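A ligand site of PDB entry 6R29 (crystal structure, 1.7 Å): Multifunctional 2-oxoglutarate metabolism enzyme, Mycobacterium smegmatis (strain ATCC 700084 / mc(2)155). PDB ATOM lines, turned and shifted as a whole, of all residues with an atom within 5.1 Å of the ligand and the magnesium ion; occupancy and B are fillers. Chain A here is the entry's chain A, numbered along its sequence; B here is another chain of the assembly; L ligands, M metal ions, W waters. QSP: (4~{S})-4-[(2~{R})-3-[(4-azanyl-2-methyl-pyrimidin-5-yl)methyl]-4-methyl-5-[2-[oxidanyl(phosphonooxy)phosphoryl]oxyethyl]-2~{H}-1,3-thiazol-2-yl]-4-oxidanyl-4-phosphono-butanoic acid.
The side-chain hydroxyl (OG) of Ser 245 lies within hydrogen-bond range of an oxygen (O15) of the ligand, 2.7 Å away. O2A of the ligand sits at hydrogen-bond distance from N of Ala 288. A ring nitrogen (NE2) of His 220 lies within hydrogen-bond range of an oxygen (O16) of the ligand (2.8 Å). An oxygen (O3B) of the ligand lies within hydrogen-bond range of a ring nitrogen (NE2) of His 180 (2.7 Å). The guanidinium group of Arg 181 is in salt-bridge range of an oxygen (O3B) of the ligand. A nitrogen (N4') of the ligand is in hydrogen-bond range of the backbone carbonyl oxygen (O) of Ser 245, 2.8 Å away. N of Asp 286 lies close to O1A of the ligand (3.5 Å). An oxygen (O2A) of the ligand is in hydrogen-bond range of the backbone NH (N) of Ala 287, 3.5 Å away. O6 of the ligand lies close to OE1 of Gln 617 of chain B (2.6 Å). A ring nitrogen (NE2) of His 661 of chain B lies within hydrogen-bond range of an oxygen (O5) of the ligand (2.7 Å). N3' of the ligand sits at hydrogen-bond distance from N of Leu 247. The side-chain carboxylate (OE1) of Glu 593 of chain B is in hydrogen-bond range of a nitrogen (N1') of the ligand, at 2.6 Å. An oxygen (O8) of the ligand sits at hydrogen-bond distance from a ring nitrogen (NE2) of His 388.
OD2 of Asp 543 of chain B sits at hydrogen-bond distance from NE2 of Gln 617 of chain B (2.9 Å). N of Gln 320 sits at hydrogen-bond distance from OD2 of Asp 286, 3.4 Å away. OG of Ser 245 sits close to NE2 of His 220, at 3.2 Å. NE2 of Gln 617 of chain B is in hydrogen-bond range of O of Gln 542 of chain B. O of His 388 is in hydrogen-bond range of NH2 of Arg 181, at 3.0 Å. OE1 of Glu 593 of chain B sits at hydrogen-bond distance from NE2 of Gln 542 of chain B (2.9 Å). The side-chain carboxylate (OE2) of Glu 593 of chain B is in hydrogen-bond range of the side-chain amide nitrogen (NE2) of Gln 292 (3.0 Å). O of Leu 591 of chain B sits at hydrogen-bond distance from NE2 of Gln 292, 2.9 Å away.
Merely in contact with the ligand: Phe 147, Tyr 219, His 246, Gly 285, Gln 292, Gly 322, Phe 323, Gln 542 of chain B, Leu 591 of chain B, Phe 618 of chain B and Phe 621 of chain B. Along chain A the residues within 4 Å of the ligand span positions 147 to 388.
Three residues have an atom within 4 Å of the magnesium ion: Asp 286, Asn 319 and Ile 321.
The magnesium ion is bound by O1A of the ligand, O2B of the ligand, OD1 of Asp 286, OD1 of Asn 319, O of Ile 321 and water W9. The magnesium ion has six donor atoms within binding distance.
Water W9 lies within hydrogen-bond range of O of Val 317 (2.7 Å), O1B of the ligand (2.8 Å), N of Asp 286 (3.3 Å) and ND2 of Asn 319 (3.4 Å). Water W3 bridges O16 of the ligand (2.7 Å) and ND1 of His 180 (2.9 Å). Water W6 lies within hydrogen-bond range of O5 of the ligand (2.7 Å), NZ of Lys 145 (3.1 Å) and OH of Tyr 219 (3.3 Å). Water W4 lies within hydrogen-bond range of an oxygen (O5) of the ligand (2.7 Å) and the side-chain amino group (NZ) of Lys 145 (2.8 Å). Water W8 bridges O2A of the ligand (2.8 Å) and N of Gly 285 (3.4 Å). Water W2 lies within hydrogen-bond range of ND1 of His 388 (2.8 Å), N of Phe 323 (2.8 Å) and O3B of the ligand (3.2 Å).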
ATOM      1  N   LYS A 145     -12.868 -29.105 -17.572  1.00  0.00           N
ATOM      2  CA  LYS A 145     -11.938 -28.869 -18.685  1.00  0.00           C
ATOM      3  C   LYS A 145     -11.225 -30.159 -19.072  1.00  0.00           C
ATOM      4  O   LYS A 145     -10.833 -30.928 -18.201  1.00  0.00           O
ATOM      5  CB  LYS A 145     -10.876 -27.827 -18.282  1.00  0.00           C
ATOM      6  CG  LYS A 145     -11.431 -26.417 -18.122  1.00  0.00           C
ATOM      7  CD  LYS A 145     -10.313 -25.379 -18.077  1.00  0.00           C
ATOM      8  CE  LYS A 145      -9.864 -25.088 -16.668  1.00  0.00           C
ATOM      9  NZ  LYS A 145      -9.556 -23.659 -16.504  1.00  0.00           N
ATOM     10  N   PHE A 147      -9.564 -30.044 -22.608  1.00  0.00           N
ATOM     11  CA  PHE A 147      -8.741 -29.631 -23.762  1.00  0.00           C
ATOM     12  C   PHE A 147      -8.802 -30.688 -24.877  1.00  0.00           C
ATOM     13  O   PHE A 147      -7.803 -31.236 -25.332  1.00  0.00           O
ATOM     14  CB  PHE A 147      -7.303 -29.300 -23.360  1.00  0.00           C
ATOM     15  CG  PHE A 147      -7.246 -28.056 -22.501  1.00  0.00           C
ATOM     16  CD1 PHE A 147      -7.613 -26.815 -23.028  1.00  0.00           C
ATOM     17  CD2 PHE A 147      -6.875 -28.119 -21.176  1.00  0.00           C
ATOM     18  CE1 PHE A 147      -7.543 -25.658 -22.247  1.00  0.00           C
ATOM     19  CE2 PHE A 147      -6.788 -26.950 -20.388  1.00  0.00           C
ATOM     20  CZ  PHE A 147      -7.135 -25.726 -20.929  1.00  0.00           C
ATOM     21  N   HIS A 180      -1.377 -29.429 -23.640  1.00  0.00           N
ATOM     22  CA  HIS A 180      -2.706 -29.842 -23.198  1.00  0.00           C
ATOM     23  C   HIS A 180      -3.615 -30.432 -24.282  1.00  0.00           C
ATOM     24  O   HIS A 180      -4.523 -31.213 -23.956  1.00  0.00           O
ATOM     25  CB  HIS A 180      -3.430 -28.608 -22.613  1.00  0.00           C
ATOM     26  CG  HIS A 180      -3.369 -27.406 -23.508  1.00  0.00           C
ATOM     27  ND1 HIS A 180      -2.182 -26.716 -23.713  1.00  0.00           N
ATOM     28  CD2 HIS A 180      -4.315 -26.875 -24.316  1.00  0.00           C
ATOM     29  CE1 HIS A 180      -2.444 -25.775 -24.613  1.00  0.00           C
ATOM     30  NE2 HIS A 180      -3.730 -25.820 -25.003  1.00  0.00           N
ATOM     31  N   ARG A 181      -3.438 -29.993 -25.551  1.00  0.00           N
ATOM     32  CA  ARG A 181      -4.395 -30.297 -26.620  1.00  0.00           C
ATOM     33  C   ARG A 181      -4.388 -31.786 -26.961  1.00  0.00           C
ATOM     34  O   ARG A 181      -3.398 -32.293 -27.459  1.00  0.00           O
ATOM     35  CB  ARG A 181      -4.088 -29.414 -27.852  1.00  0.00           C
ATOM     36  CG  ARG A 181      -5.146 -29.460 -28.951  1.00  0.00           C
ATOM     37  CD  ARG A 181      -6.510 -28.969 -28.469  1.00  0.00           C
ATOM     38  NE  ARG A 181      -6.482 -27.601 -27.917  1.00  0.00           N
ATOM     39  CZ  ARG A 181      -7.472 -27.047 -27.229  1.00  0.00           C
ATOM     40  NH1 ARG A 181      -8.594 -27.738 -26.997  1.00  0.00           N
ATOM     41  NH2 ARG A 181      -7.368 -25.818 -26.755  1.00  0.00           N
ATOM     42  N   TYR A 219      -4.222 -33.024 -17.176  1.00  0.00           N
ATOM     43  CA  TYR A 219      -3.664 -32.819 -18.513  1.00  0.00           C
ATOM     44  C   TYR A 219      -2.164 -32.411 -18.459  1.00  0.00           C
ATOM     45  O   TYR A 219      -1.634 -31.925 -19.468  1.00  0.00           O
ATOM     46  CB  TYR A 219      -4.547 -31.813 -19.319  1.00  0.00           C
ATOM     47  CG  TYR A 219      -4.876 -30.533 -18.598  1.00  0.00           C
ATOM     48  CD1 TYR A 219      -4.020 -29.451 -18.647  1.00  0.00           C
ATOM     49  CD2 TYR A 219      -6.079 -30.386 -17.893  1.00  0.00           C
ATOM     50  CE1 TYR A 219      -4.314 -28.266 -17.974  1.00  0.00           C
ATOM     51  CE2 TYR A 219      -6.370 -29.211 -17.197  1.00  0.00           C
ATOM     52  CZ  TYR A 219      -5.489 -28.146 -17.249  1.00  0.00           C
ATOM     53  OH  TYR A 219      -5.740 -26.975 -16.569  1.00  0.00           O
ATOM     54  N   HIS A 220      -1.481 -32.656 -17.313  1.00  0.00           N
ATOM     55  CA  HIS A 220      -0.028 -32.439 -17.164  1.00  0.00           C
ATOM     56  C   HIS A 220       0.693 -33.753 -16.876  1.00  0.00           C
ATOM     57  O   HIS A 220       1.914 -33.753 -16.702  1.00  0.00           O
ATOM     58  CB  HIS A 220       0.244 -31.472 -16.000  1.00  0.00           C
ATOM     59  CG  HIS A 220      -0.091 -30.050 -16.302  1.00  0.00           C
ATOM     60  ND1 HIS A 220       0.082 -29.053 -15.351  1.00  0.00           N
ATOM     61  CD2 HIS A 220      -0.603 -29.496 -17.438  1.00  0.00           C
ATOM     62  CE1 HIS A 220      -0.338 -27.930 -15.921  1.00  0.00           C
ATOM     63  NE2 HIS A 220      -0.750 -28.137 -17.188  1.00  0.00           N
ATOM     64  N   PRO A 244       4.647 -28.705 -16.759  1.00  0.00           N
ATOM     65  CA  PRO A 244       3.817 -27.671 -16.116  1.00  0.00           C
ATOM     66  C   PRO A 244       2.905 -27.018 -17.171  1.00  0.00           C
ATOM     67  O   PRO A 244       2.974 -27.365 -18.390  1.00  0.00           O
ATOM     68  CB  PRO A 244       4.864 -26.673 -15.614  1.00  0.00           C
ATOM     69  CG  PRO A 244       5.932 -26.720 -16.726  1.00  0.00           C
ATOM     70  CD  PRO A 244       5.976 -28.182 -17.136  1.00  0.00           C
ATOM     71  N   SER A 245       2.081 -26.028 -16.758  1.00  0.00           N
ATOM     72  CA  SER A 245       1.248 -25.324 -17.732  1.00  0.00           C
ATOM     73  C   SER A 245       2.095 -24.537 -18.735  1.00  0.00           C
ATOM     74  O   SER A 245       1.654 -24.357 -19.861  1.00  0.00           O
ATOM     75  CB  SER A 245       0.307 -24.349 -17.043  1.00  0.00           C
ATOM     76  OG  SER A 245      -0.761 -25.060 -16.420  1.00  0.00           O
ATOM     77  N   HIS A 246       3.275 -24.044 -18.297  1.00  0.00           N
ATOM     78  CA  HIS A 246       4.159 -23.184 -19.104  1.00  0.00           C
ATOM     79  C   HIS A 246       4.485 -23.835 -20.436  1.00  0.00           C
ATOM     80  O   HIS A 246       5.260 -24.778 -20.496  1.00  0.00           O
ATOM     81  CB  HIS A 246       5.424 -22.848 -18.328  1.00  0.00           C
ATOM     82  CG  HIS A 246       5.146 -22.067 -17.073  1.00  0.00           C
ATOM     83  ND1 HIS A 246       4.288 -22.532 -16.102  1.00  0.00           N
ATOM     84  CD2 HIS A 246       5.635 -20.848 -16.699  1.00  0.00           C
ATOM     85  CE1 HIS A 246       4.234 -21.569 -15.172  1.00  0.00           C
ATOM     86  NE2 HIS A 246       5.053 -20.558 -15.472  1.00  0.00           N
ATOM     87  N   LEU A 247       3.829 -23.345 -21.496  1.00  0.00           N
ATOM     88  CA  LEU A 247       3.948 -23.996 -22.806  1.00  0.00           C
ATOM     89  C   LEU A 247       5.362 -23.933 -23.329  1.00  0.00           C
ATOM     90  O   LEU A 247       6.055 -22.910 -23.213  1.00  0.00           O
ATOM     91  CB  LEU A 247       2.979 -23.332 -23.808  1.00  0.00           C
ATOM     92  CG  LEU A 247       1.490 -23.415 -23.384  1.00  0.00           C
ATOM     93  CD1 LEU A 247       0.626 -22.456 -24.219  1.00  0.00           C
ATOM     94  CD2 LEU A 247       0.960 -24.859 -23.512  1.00  0.00           C
ATOM     95  N   GLY A 285       1.515 -26.511 -29.760  1.00  0.00           N
ATOM     96  CA  GLY A 285       0.365 -25.734 -30.252  1.00  0.00           C
ATOM     97  C   GLY A 285       0.887 -24.663 -31.204  1.00  0.00           C
ATOM     98  O   GLY A 285       2.065 -24.274 -31.112  1.00  0.00           O
ATOM     99  N   ASP A 286       0.035 -24.135 -32.103  1.00  0.00           N
ATOM    100  CA  ASP A 286       0.498 -23.144 -33.097  1.00  0.00           C
ATOM    101  C   ASP A 286       0.870 -21.796 -32.468  1.00  0.00           C
ATOM    102  O   ASP A 286       1.861 -21.181 -32.881  1.00  0.00           O
ATOM    103  CB  ASP A 286      -0.520 -22.919 -34.222  1.00  0.00           C
ATOM    104  CG  ASP A 286      -1.938 -22.598 -33.766  1.00  0.00           C
ATOM    105  OD1 ASP A 286      -2.481 -23.375 -32.962  1.00  0.00           O
ATOM    106  OD2 ASP A 286      -2.508 -21.621 -34.270  1.00  0.00           O
ATOM    107  N   ALA A 287       0.071 -21.290 -31.519  1.00  0.00           N
ATOM    108  CA  ALA A 287       0.412 -19.976 -30.960  1.00  0.00           C
ATOM    109  C   ALA A 287       1.686 -20.075 -30.087  1.00  0.00           C
ATOM    110  O   ALA A 287       2.564 -19.211 -30.168  1.00  0.00           O
ATOM    111  CB  ALA A 287      -0.774 -19.424 -30.149  1.00  0.00           C
ATOM    112  N   ALA A 288       1.790 -21.148 -29.287  1.00  0.00           N
ATOM    113  CA  ALA A 288       2.960 -21.313 -28.430  1.00  0.00           C
ATOM    114  C   ALA A 288       4.251 -21.545 -29.235  1.00  0.00           C
ATOM    115  O   ALA A 288       5.313 -21.039 -28.835  1.00  0.00           O
ATOM    116  CB  ALA A 288       2.734 -22.481 -27.471  1.00  0.00           C
ATOM    117  N   PHE A 289       4.192 -22.330 -30.317  1.00  0.00           N
ATOM    118  CA  PHE A 289       5.410 -22.646 -31.051  1.00  0.00           C
ATOM    119  C   PHE A 289       6.048 -21.384 -31.623  1.00  0.00           C
ATOM    120  O   PHE A 289       7.280 -21.267 -31.641  1.00  0.00           O
ATOM    121  CB  PHE A 289       5.106 -23.649 -32.156  1.00  0.00           C
ATOM    122  CG  PHE A 289       6.334 -24.342 -32.712  1.00  0.00           C
ATOM    123  CD1 PHE A 289       7.100 -25.183 -31.919  1.00  0.00           C
ATOM    124  CD2 PHE A 289       6.721 -24.143 -34.033  1.00  0.00           C
ATOM    125  CE1 PHE A 289       8.214 -25.863 -32.445  1.00  0.00           C
ATOM    126  CE2 PHE A 289       7.843 -24.812 -34.556  1.00  0.00           C
ATOM    127  CZ  PHE A 289       8.551 -25.692 -33.768  1.00  0.00           C
ATOM    128  N   GLN A 292       7.034 -18.581 -27.981  1.00  0.00           N
ATOM    129  CA  GLN A 292       7.937 -18.853 -26.853  1.00  0.00           C
ATOM    130  C   GLN A 292       9.382 -18.999 -27.305  1.00  0.00           C
ATOM    131  O   GLN A 292       9.678 -19.888 -28.105  1.00  0.00           O
ATOM    132  CB  GLN A 292       7.458 -20.145 -26.131  1.00  0.00           C
ATOM    133  CG  GLN A 292       6.142 -19.916 -25.369  1.00  0.00           C
ATOM    134  CD  GLN A 292       6.363 -19.060 -24.126  1.00  0.00           C
ATOM    135  OE1 GLN A 292       7.242 -19.349 -23.293  1.00  0.00           O
ATOM    136  NE2 GLN A 292       5.581 -18.008 -23.984  1.00  0.00           N
ATOM    137  N   VAL A 317       0.068 -29.155 -33.658  1.00  0.00           N
ATOM    138  CA  VAL A 317      -1.394 -29.303 -33.783  1.00  0.00           C
ATOM    139  C   VAL A 317      -1.882 -27.903 -34.107  1.00  0.00           C
ATOM    140  O   VAL A 317      -2.127 -27.069 -33.203  1.00  0.00           O
ATOM    141  CB  VAL A 317      -2.020 -29.921 -32.509  1.00  0.00           C
ATOM    142  CG1 VAL A 317      -3.538 -30.016 -32.675  1.00  0.00           C
ATOM    143  CG2 VAL A 317      -1.420 -31.303 -32.223  1.00  0.00           C
ATOM    144  N   ASN A 319      -4.341 -25.646 -35.032  1.00  0.00           N
ATOM    145  CA  ASN A 319      -5.794 -25.429 -35.122  1.00  0.00           C
ATOM    146  C   ASN A 319      -6.134 -23.965 -35.477  1.00  0.00           C
ATOM    147  O   ASN A 319      -7.296 -23.527 -35.372  1.00  0.00           O
ATOM    148  CB  ASN A 319      -6.493 -25.896 -33.856  1.00  0.00           C
ATOM    149  CG  ASN A 319      -5.897 -25.347 -32.591  1.00  0.00           C
ATOM    150  OD1 ASN A 319      -5.177 -24.347 -32.629  1.00  0.00           O
ATOM    151  ND2 ASN A 319      -6.182 -25.992 -31.461  1.00  0.00           N
ATOM    152  N   GLN A 320      -5.098 -23.182 -35.923  1.00  0.00           N
ATOM    153  CA  GLN A 320      -5.275 -21.831 -36.469  1.00  0.00           C
ATOM    154  C   GLN A 320      -5.957 -20.883 -35.478  1.00  0.00           C
ATOM    155  O   GLN A 320      -6.684 -19.963 -35.878  1.00  0.00           O
ATOM    156  CB  GLN A 320      -6.059 -21.921 -37.805  1.00  0.00           C
ATOM    157  CG  GLN A 320      -5.482 -23.028 -38.702  1.00  0.00           C
ATOM    158  CD  GLN A 320      -6.189 -23.107 -40.016  1.00  0.00           C
ATOM    159  OE1 GLN A 320      -6.067 -22.211 -40.824  1.00  0.00           O
ATOM    160  NE2 GLN A 320      -6.943 -24.197 -40.251  1.00  0.00           N
ATOM    161  N   ILE A 321      -5.676 -21.102 -34.172  1.00  0.00           N
ATOM    162  CA  ILE A 321      -6.218 -20.266 -33.088  1.00  0.00           C
ATOM    163  C   ILE A 321      -5.368 -20.538 -31.863  1.00  0.00           C
ATOM    164  O   ILE A 321      -4.845 -21.636 -31.694  1.00  0.00           O
ATOM    165  CB  ILE A 321      -7.730 -20.581 -32.867  1.00  0.00           C
ATOM    166  CG1 ILE A 321      -8.418 -19.490 -31.986  1.00  0.00           C
ATOM    167  CG2 ILE A 321      -7.953 -22.013 -32.310  1.00  0.00           C
ATOM    168  CD1 ILE A 321      -9.893 -19.468 -32.112  1.00  0.00           C
ATOM    169  N   GLY A 322      -5.290 -19.544 -30.995  1.00  0.00           N
ATOM    170  CA  GLY A 322      -4.653 -19.718 -29.689  1.00  0.00           C
ATOM    171  C   GLY A 322      -5.588 -19.042 -28.685  1.00  0.00           C
ATOM    172  O   GLY A 322      -5.513 -17.831 -28.496  1.00  0.00           O
ATOM    173  N   PHE A 323      -6.498 -19.820 -28.077  1.00  0.00           N
ATOM    174  CA  PHE A 323      -7.532 -19.350 -27.133  1.00  0.00           C
ATOM    175  C   PHE A 323      -8.482 -18.394 -27.917  1.00  0.00           C
ATOM    176  O   PHE A 323      -9.261 -18.899 -28.722  1.00  0.00           O
ATOM    177  CB  PHE A 323      -6.888 -18.702 -25.884  1.00  0.00           C
ATOM    178  CG  PHE A 323      -7.793 -18.583 -24.665  1.00  0.00           C
ATOM    179  CD1 PHE A 323      -9.180 -18.628 -24.793  1.00  0.00           C
ATOM    180  CD2 PHE A 323      -7.245 -18.487 -23.394  1.00  0.00           C
ATOM    181  CE1 PHE A 323     -10.005 -18.565 -23.665  1.00  0.00           C
ATOM    182  CE2 PHE A 323      -8.074 -18.394 -22.265  1.00  0.00           C
ATOM    183  CZ  PHE A 323      -9.443 -18.426 -22.417  1.00  0.00           C
ATOM    184  N   HIS A 388     -11.914 -22.870 -26.505  1.00  0.00           N
ATOM    185  CA  HIS A 388     -10.547 -23.158 -26.066  1.00  0.00           C
ATOM    186  C   HIS A 388     -10.518 -24.259 -25.006  1.00  0.00           C
ATOM    187  O   HIS A 388      -9.704 -25.186 -25.059  1.00  0.00           O
ATOM    188  CB  HIS A 388      -9.928 -21.882 -25.503  1.00  0.00           C
ATOM    189  CG  HIS A 388      -8.568 -22.103 -24.941  1.00  0.00           C
ATOM    190  ND1 HIS A 388      -7.542 -22.660 -25.711  1.00  0.00           N
ATOM    191  CD2 HIS A 388      -8.087 -21.845 -23.695  1.00  0.00           C
ATOM    192  CE1 HIS A 388      -6.493 -22.710 -24.917  1.00  0.00           C
ATOM    193  NE2 HIS A 388      -6.773 -22.223 -23.688  1.00  0.00           N
ATOM    194  N   GLN B 542      -2.309 -11.574 -23.088  1.00  0.00           N
ATOM    195  CA  GLN B 542      -2.894 -12.731 -23.768  1.00  0.00           C
ATOM    196  C   GLN B 542      -4.404 -12.751 -23.598  1.00  0.00           C
ATOM    197  O   GLN B 542      -4.916 -12.742 -22.463  1.00  0.00           O
ATOM    198  CB  GLN B 542      -2.252 -14.040 -23.273  1.00  0.00           C
ATOM    199  CG  GLN B 542      -0.797 -14.162 -23.805  1.00  0.00           C
ATOM    200  CD  GLN B 542       0.039 -15.036 -22.910  1.00  0.00           C
ATOM    201  OE1 GLN B 542      -0.491 -15.861 -22.147  1.00  0.00           O
ATOM    202  NE2 GLN B 542       1.376 -14.893 -23.001  1.00  0.00           N
ATOM    203  N   ASP B 543      -5.099 -12.659 -24.740  1.00  0.00           N
ATOM    204  CA  ASP B 543      -6.578 -12.659 -24.827  1.00  0.00           C
ATOM    205  C   ASP B 543      -7.177 -11.472 -24.031  1.00  0.00           C
ATOM    206  O   ASP B 543      -8.337 -11.536 -23.587  1.00  0.00           O
ATOM    207  CB  ASP B 543      -7.110 -14.025 -24.339  1.00  0.00           C
ATOM    208  CG  ASP B 543      -6.450 -15.121 -25.178  1.00  0.00           C
ATOM    209  OD1 ASP B 543      -6.760 -15.202 -26.392  1.00  0.00           O
ATOM    210  OD2 ASP B 543      -5.541 -15.793 -24.670  1.00  0.00           O
ATOM    211  N   LEU B 591       1.973 -15.032 -27.831  1.00  0.00           N
ATOM    212  CA  LEU B 591       2.062 -15.923 -26.673  1.00  0.00           C
ATOM    213  C   LEU B 591       3.496 -15.919 -26.180  1.00  0.00           C
ATOM    214  O   LEU B 591       4.256 -16.883 -26.325  1.00  0.00           O
ATOM    215  CB  LEU B 591       1.600 -17.351 -27.042  1.00  0.00           C
ATOM    216  CG  LEU B 591       0.918 -18.096 -25.901  1.00  0.00           C
ATOM    217  CD1 LEU B 591       0.257 -19.358 -26.448  1.00  0.00           C
ATOM    218  CD2 LEU B 591       1.945 -18.510 -24.810  1.00  0.00           C
ATOM    219  N   GLU B 593       5.974 -13.936 -22.875  1.00  0.00           N
ATOM    220  CA  GLU B 593       5.974 -13.174 -21.625  1.00  0.00           C
ATOM    221  C   GLU B 593       7.235 -12.315 -21.622  1.00  0.00           C
ATOM    222  O   GLU B 593       7.165 -11.116 -21.397  1.00  0.00           O
ATOM    223  CB  GLU B 593       5.914 -14.059 -20.377  1.00  0.00           C
ATOM    224  CG  GLU B 593       4.506 -14.582 -20.097  1.00  0.00           C
ATOM    225  CD  GLU B 593       4.149 -15.844 -20.865  1.00  0.00           C
ATOM    226  OE1 GLU B 593       2.939 -16.158 -20.910  1.00  0.00           O
ATOM    227  OE2 GLU B 593       5.073 -16.522 -21.384  1.00  0.00           O
ATOM    228  N   GLN B 617      -1.898 -13.898 -18.459  1.00  0.00           N
ATOM    229  CA  GLN B 617      -3.148 -14.683 -18.560  1.00  0.00           C
ATOM    230  C   GLN B 617      -3.550 -15.138 -17.146  1.00  0.00           C
ATOM    231  O   GLN B 617      -4.689 -14.956 -16.705  1.00  0.00           O
ATOM    232  CB  GLN B 617      -2.984 -15.871 -19.516  1.00  0.00           C
ATOM    233  CG  GLN B 617      -4.310 -16.616 -19.635  1.00  0.00           C
ATOM    234  CD  GLN B 617      -4.649 -16.899 -21.073  1.00  0.00           C
ATOM    235  OE1 GLN B 617      -4.484 -18.017 -21.545  1.00  0.00           O
ATOM    236  NE2 GLN B 617      -5.141 -15.896 -21.792  1.00  0.00           N
ATOM    237  N   PHE B 618      -2.562 -15.682 -16.431  1.00  0.00           N
ATOM    238  CA  PHE B 618      -2.583 -15.979 -14.986  1.00  0.00           C
ATOM    239  C   PHE B 618      -1.268 -15.457 -14.488  1.00  0.00           C
ATOM    240  O   PHE B 618      -0.273 -15.553 -15.211  1.00  0.00           O
ATOM    241  CB  PHE B 618      -2.738 -17.495 -14.712  1.00  0.00           C
ATOM    242  CG  PHE B 618      -4.125 -18.012 -15.043  1.00  0.00           C
ATOM    243  CD1 PHE B 618      -4.469 -18.329 -16.356  1.00  0.00           C
ATOM    244  CD2 PHE B 618      -5.093 -18.160 -14.047  1.00  0.00           C
ATOM    245  CE1 PHE B 618      -5.753 -18.770 -16.671  1.00  0.00           C
ATOM    246  CE2 PHE B 618      -6.384 -18.591 -14.375  1.00  0.00           C
ATOM    247  CZ  PHE B 618      -6.716 -18.866 -15.679  1.00  0.00           C
ATOM    248  N   PHE B 621       2.352 -17.174 -14.956  1.00  0.00           N
ATOM    249  CA  PHE B 621       3.233 -17.208 -16.123  1.00  0.00           C
ATOM    250  C   PHE B 621       4.220 -16.036 -16.176  1.00  0.00           C
ATOM    251  O   PHE B 621       5.096 -16.045 -17.060  1.00  0.00           O
ATOM    252  CB  PHE B 621       2.380 -17.218 -17.428  1.00  0.00           C
ATOM    253  CG  PHE B 621       1.490 -18.435 -17.458  1.00  0.00           C
ATOM    254  CD1 PHE B 621       2.031 -19.709 -17.427  1.00  0.00           C
ATOM    255  CD2 PHE B 621       0.107 -18.301 -17.428  1.00  0.00           C
ATOM    256  CE1 PHE B 621       1.217 -20.844 -17.407  1.00  0.00           C
ATOM    257  CE2 PHE B 621      -0.724 -19.440 -17.340  1.00  0.00           C
ATOM    258  CZ  PHE B 621      -0.156 -20.699 -17.351  1.00  0.00           C
ATOM    259  N   HIS B 661      -2.267 -22.139 -11.876  1.00  0.00           N
ATOM    260  CA  HIS B 661      -3.429 -21.249 -12.047  1.00  0.00           C
ATOM    261  C   HIS B 661      -3.829 -20.702 -10.689  1.00  0.00           C
ATOM    262  O   HIS B 661      -5.008 -20.522 -10.407  1.00  0.00           O
ATOM    263  CB  HIS B 661      -4.609 -21.970 -12.690  1.00  0.00           C
ATOM    264  CG  HIS B 661      -4.363 -22.286 -14.125  1.00  0.00           C
ATOM    265  ND1 HIS B 661      -3.639 -23.403 -14.493  1.00  0.00           N
ATOM    266  CD2 HIS B 661      -4.779 -21.638 -15.234  1.00  0.00           C
ATOM    267  CE1 HIS B 661      -3.598 -23.368 -15.822  1.00  0.00           C
ATOM    268  NE2 HIS B 661      -4.272 -22.327 -16.309  1.00  0.00           N
HETATM  269  N1' QSP L   1       1.940 -18.588 -21.230  1.00  0.00           N
HETATM  270  C2' QSP L   1       2.565 -19.781 -21.114  1.00  0.00           C
HETATM  271  CM2 QSP L   1       4.083 -19.782 -21.196  1.00  0.00           C
HETATM  272  N3' QSP L   1       2.011 -20.972 -20.914  1.00  0.00           N
HETATM  273  C4' QSP L   1       0.640 -20.970 -20.792  1.00  0.00           C
HETATM  274  N4' QSP L   1       0.070 -22.117 -20.389  1.00  0.00           N
HETATM  275  C5' QSP L   1      -0.163 -19.753 -20.960  1.00  0.00           C
HETATM  276  C6' QSP L   1       0.555 -18.607 -21.170  1.00  0.00           C
HETATM  277  C7' QSP L   1      -1.667 -19.759 -20.883  1.00  0.00           C
HETATM  278  N3  QSP L   1      -2.378 -20.491 -21.972  1.00  0.00           N
HETATM  279  C2  QSP L   1      -2.660 -21.924 -21.788  1.00  0.00           C
HETATM  280  S1  QSP L   1      -3.402 -22.436 -23.414  1.00  0.00           S
HETATM  281  C5  QSP L   1      -2.974 -20.897 -24.203  1.00  0.00           C
HETATM  282  C4  QSP L   1      -2.445 -20.007 -23.329  1.00  0.00           C
HETATM  283  CM4 QSP L   1      -2.026 -18.611 -23.665  1.00  0.00           C
HETATM  284  C6  QSP L   1      -3.220 -20.752 -25.642  1.00  0.00           C
HETATM  285  C7  QSP L   1      -2.368 -21.738 -26.478  1.00  0.00           C
HETATM  286  O7  QSP L   1      -2.685 -21.706 -27.815  1.00  0.00           O
HETATM  287  PA  QSP L   1      -1.961 -22.830 -28.793  1.00  0.00           P
HETATM  288  O1A QSP L   1      -2.358 -22.476 -30.180  1.00  0.00           O
HETATM  289  O2A QSP L   1      -0.503 -22.888 -28.514  1.00  0.00           O
HETATM  290  O3A QSP L   1      -2.594 -24.151 -28.290  1.00  0.00           O
HETATM  291  PB  QSP L   1      -4.207 -24.686 -28.423  1.00  0.00           P
HETATM  292  O1B QSP L   1      -4.088 -26.148 -28.726  1.00  0.00           O
HETATM  293  O2B QSP L   1      -4.799 -23.911 -29.573  1.00  0.00           O
HETATM  294  O3B QSP L   1      -4.853 -24.428 -27.085  1.00  0.00           O
HETATM  295  C11 QSP L   1      -3.437 -22.402 -20.566  1.00  0.00           C
HETATM  296  P4  QSP L   1      -5.019 -21.449 -20.038  1.00  0.00           P
HETATM  297  O5  QSP L   1      -5.459 -22.050 -18.718  1.00  0.00           O
HETATM  298  O6  QSP L   1      -4.555 -20.008 -19.808  1.00  0.00           O
HETATM  299  O8  QSP L   1      -6.046 -21.611 -21.145  1.00  0.00           O
HETATM  300  C12 QSP L   1      -3.881 -23.902 -20.749  1.00  0.00           C
HETATM  301  O11 QSP L   1      -2.569 -22.304 -19.454  1.00  0.00           O
HETATM  302  C13 QSP L   1      -2.734 -24.951 -20.771  1.00  0.00           C
HETATM  303  C14 QSP L   1      -2.311 -25.434 -19.352  1.00  0.00           C
HETATM  304  O15 QSP L   1      -2.612 -24.743 -18.321  1.00  0.00           O
HETATM  305  O16 QSP L   1      -1.678 -26.504 -19.243  1.00  0.00           O
HETATM  306 MG    MG M   1      -3.789 -23.447 -31.330  1.00  0.00          MG
HETATM  307  O   HOH W   1      -1.656 -27.179 -27.632  1.00  0.00           O
HETATM  308  O   HOH W   2      -7.018 -22.591 -28.477  1.00  0.00           O
HETATM  309  O   HOH W   3      -0.466 -27.314 -21.458  1.00  0.00           O
HETATM  310  O   HOH W   4      -7.932 -21.659 -17.644  1.00  0.00           O
HETATM  311  O   HOH W   5      -8.512 -22.308 -20.237  1.00  0.00           O
HETATM  312  O   HOH W   6      -6.839 -24.149 -17.855  1.00  0.00           O
HETATM  313  O   HOH W   7       5.860 -17.943 -18.946  1.00  0.00           O
HETATM  314  O   HOH W   8       0.165 -25.137 -26.978  1.00  0.00           O
HETATM  315  O   HOH W   9      -2.886 -25.438 -31.164  1.00  0.00           O
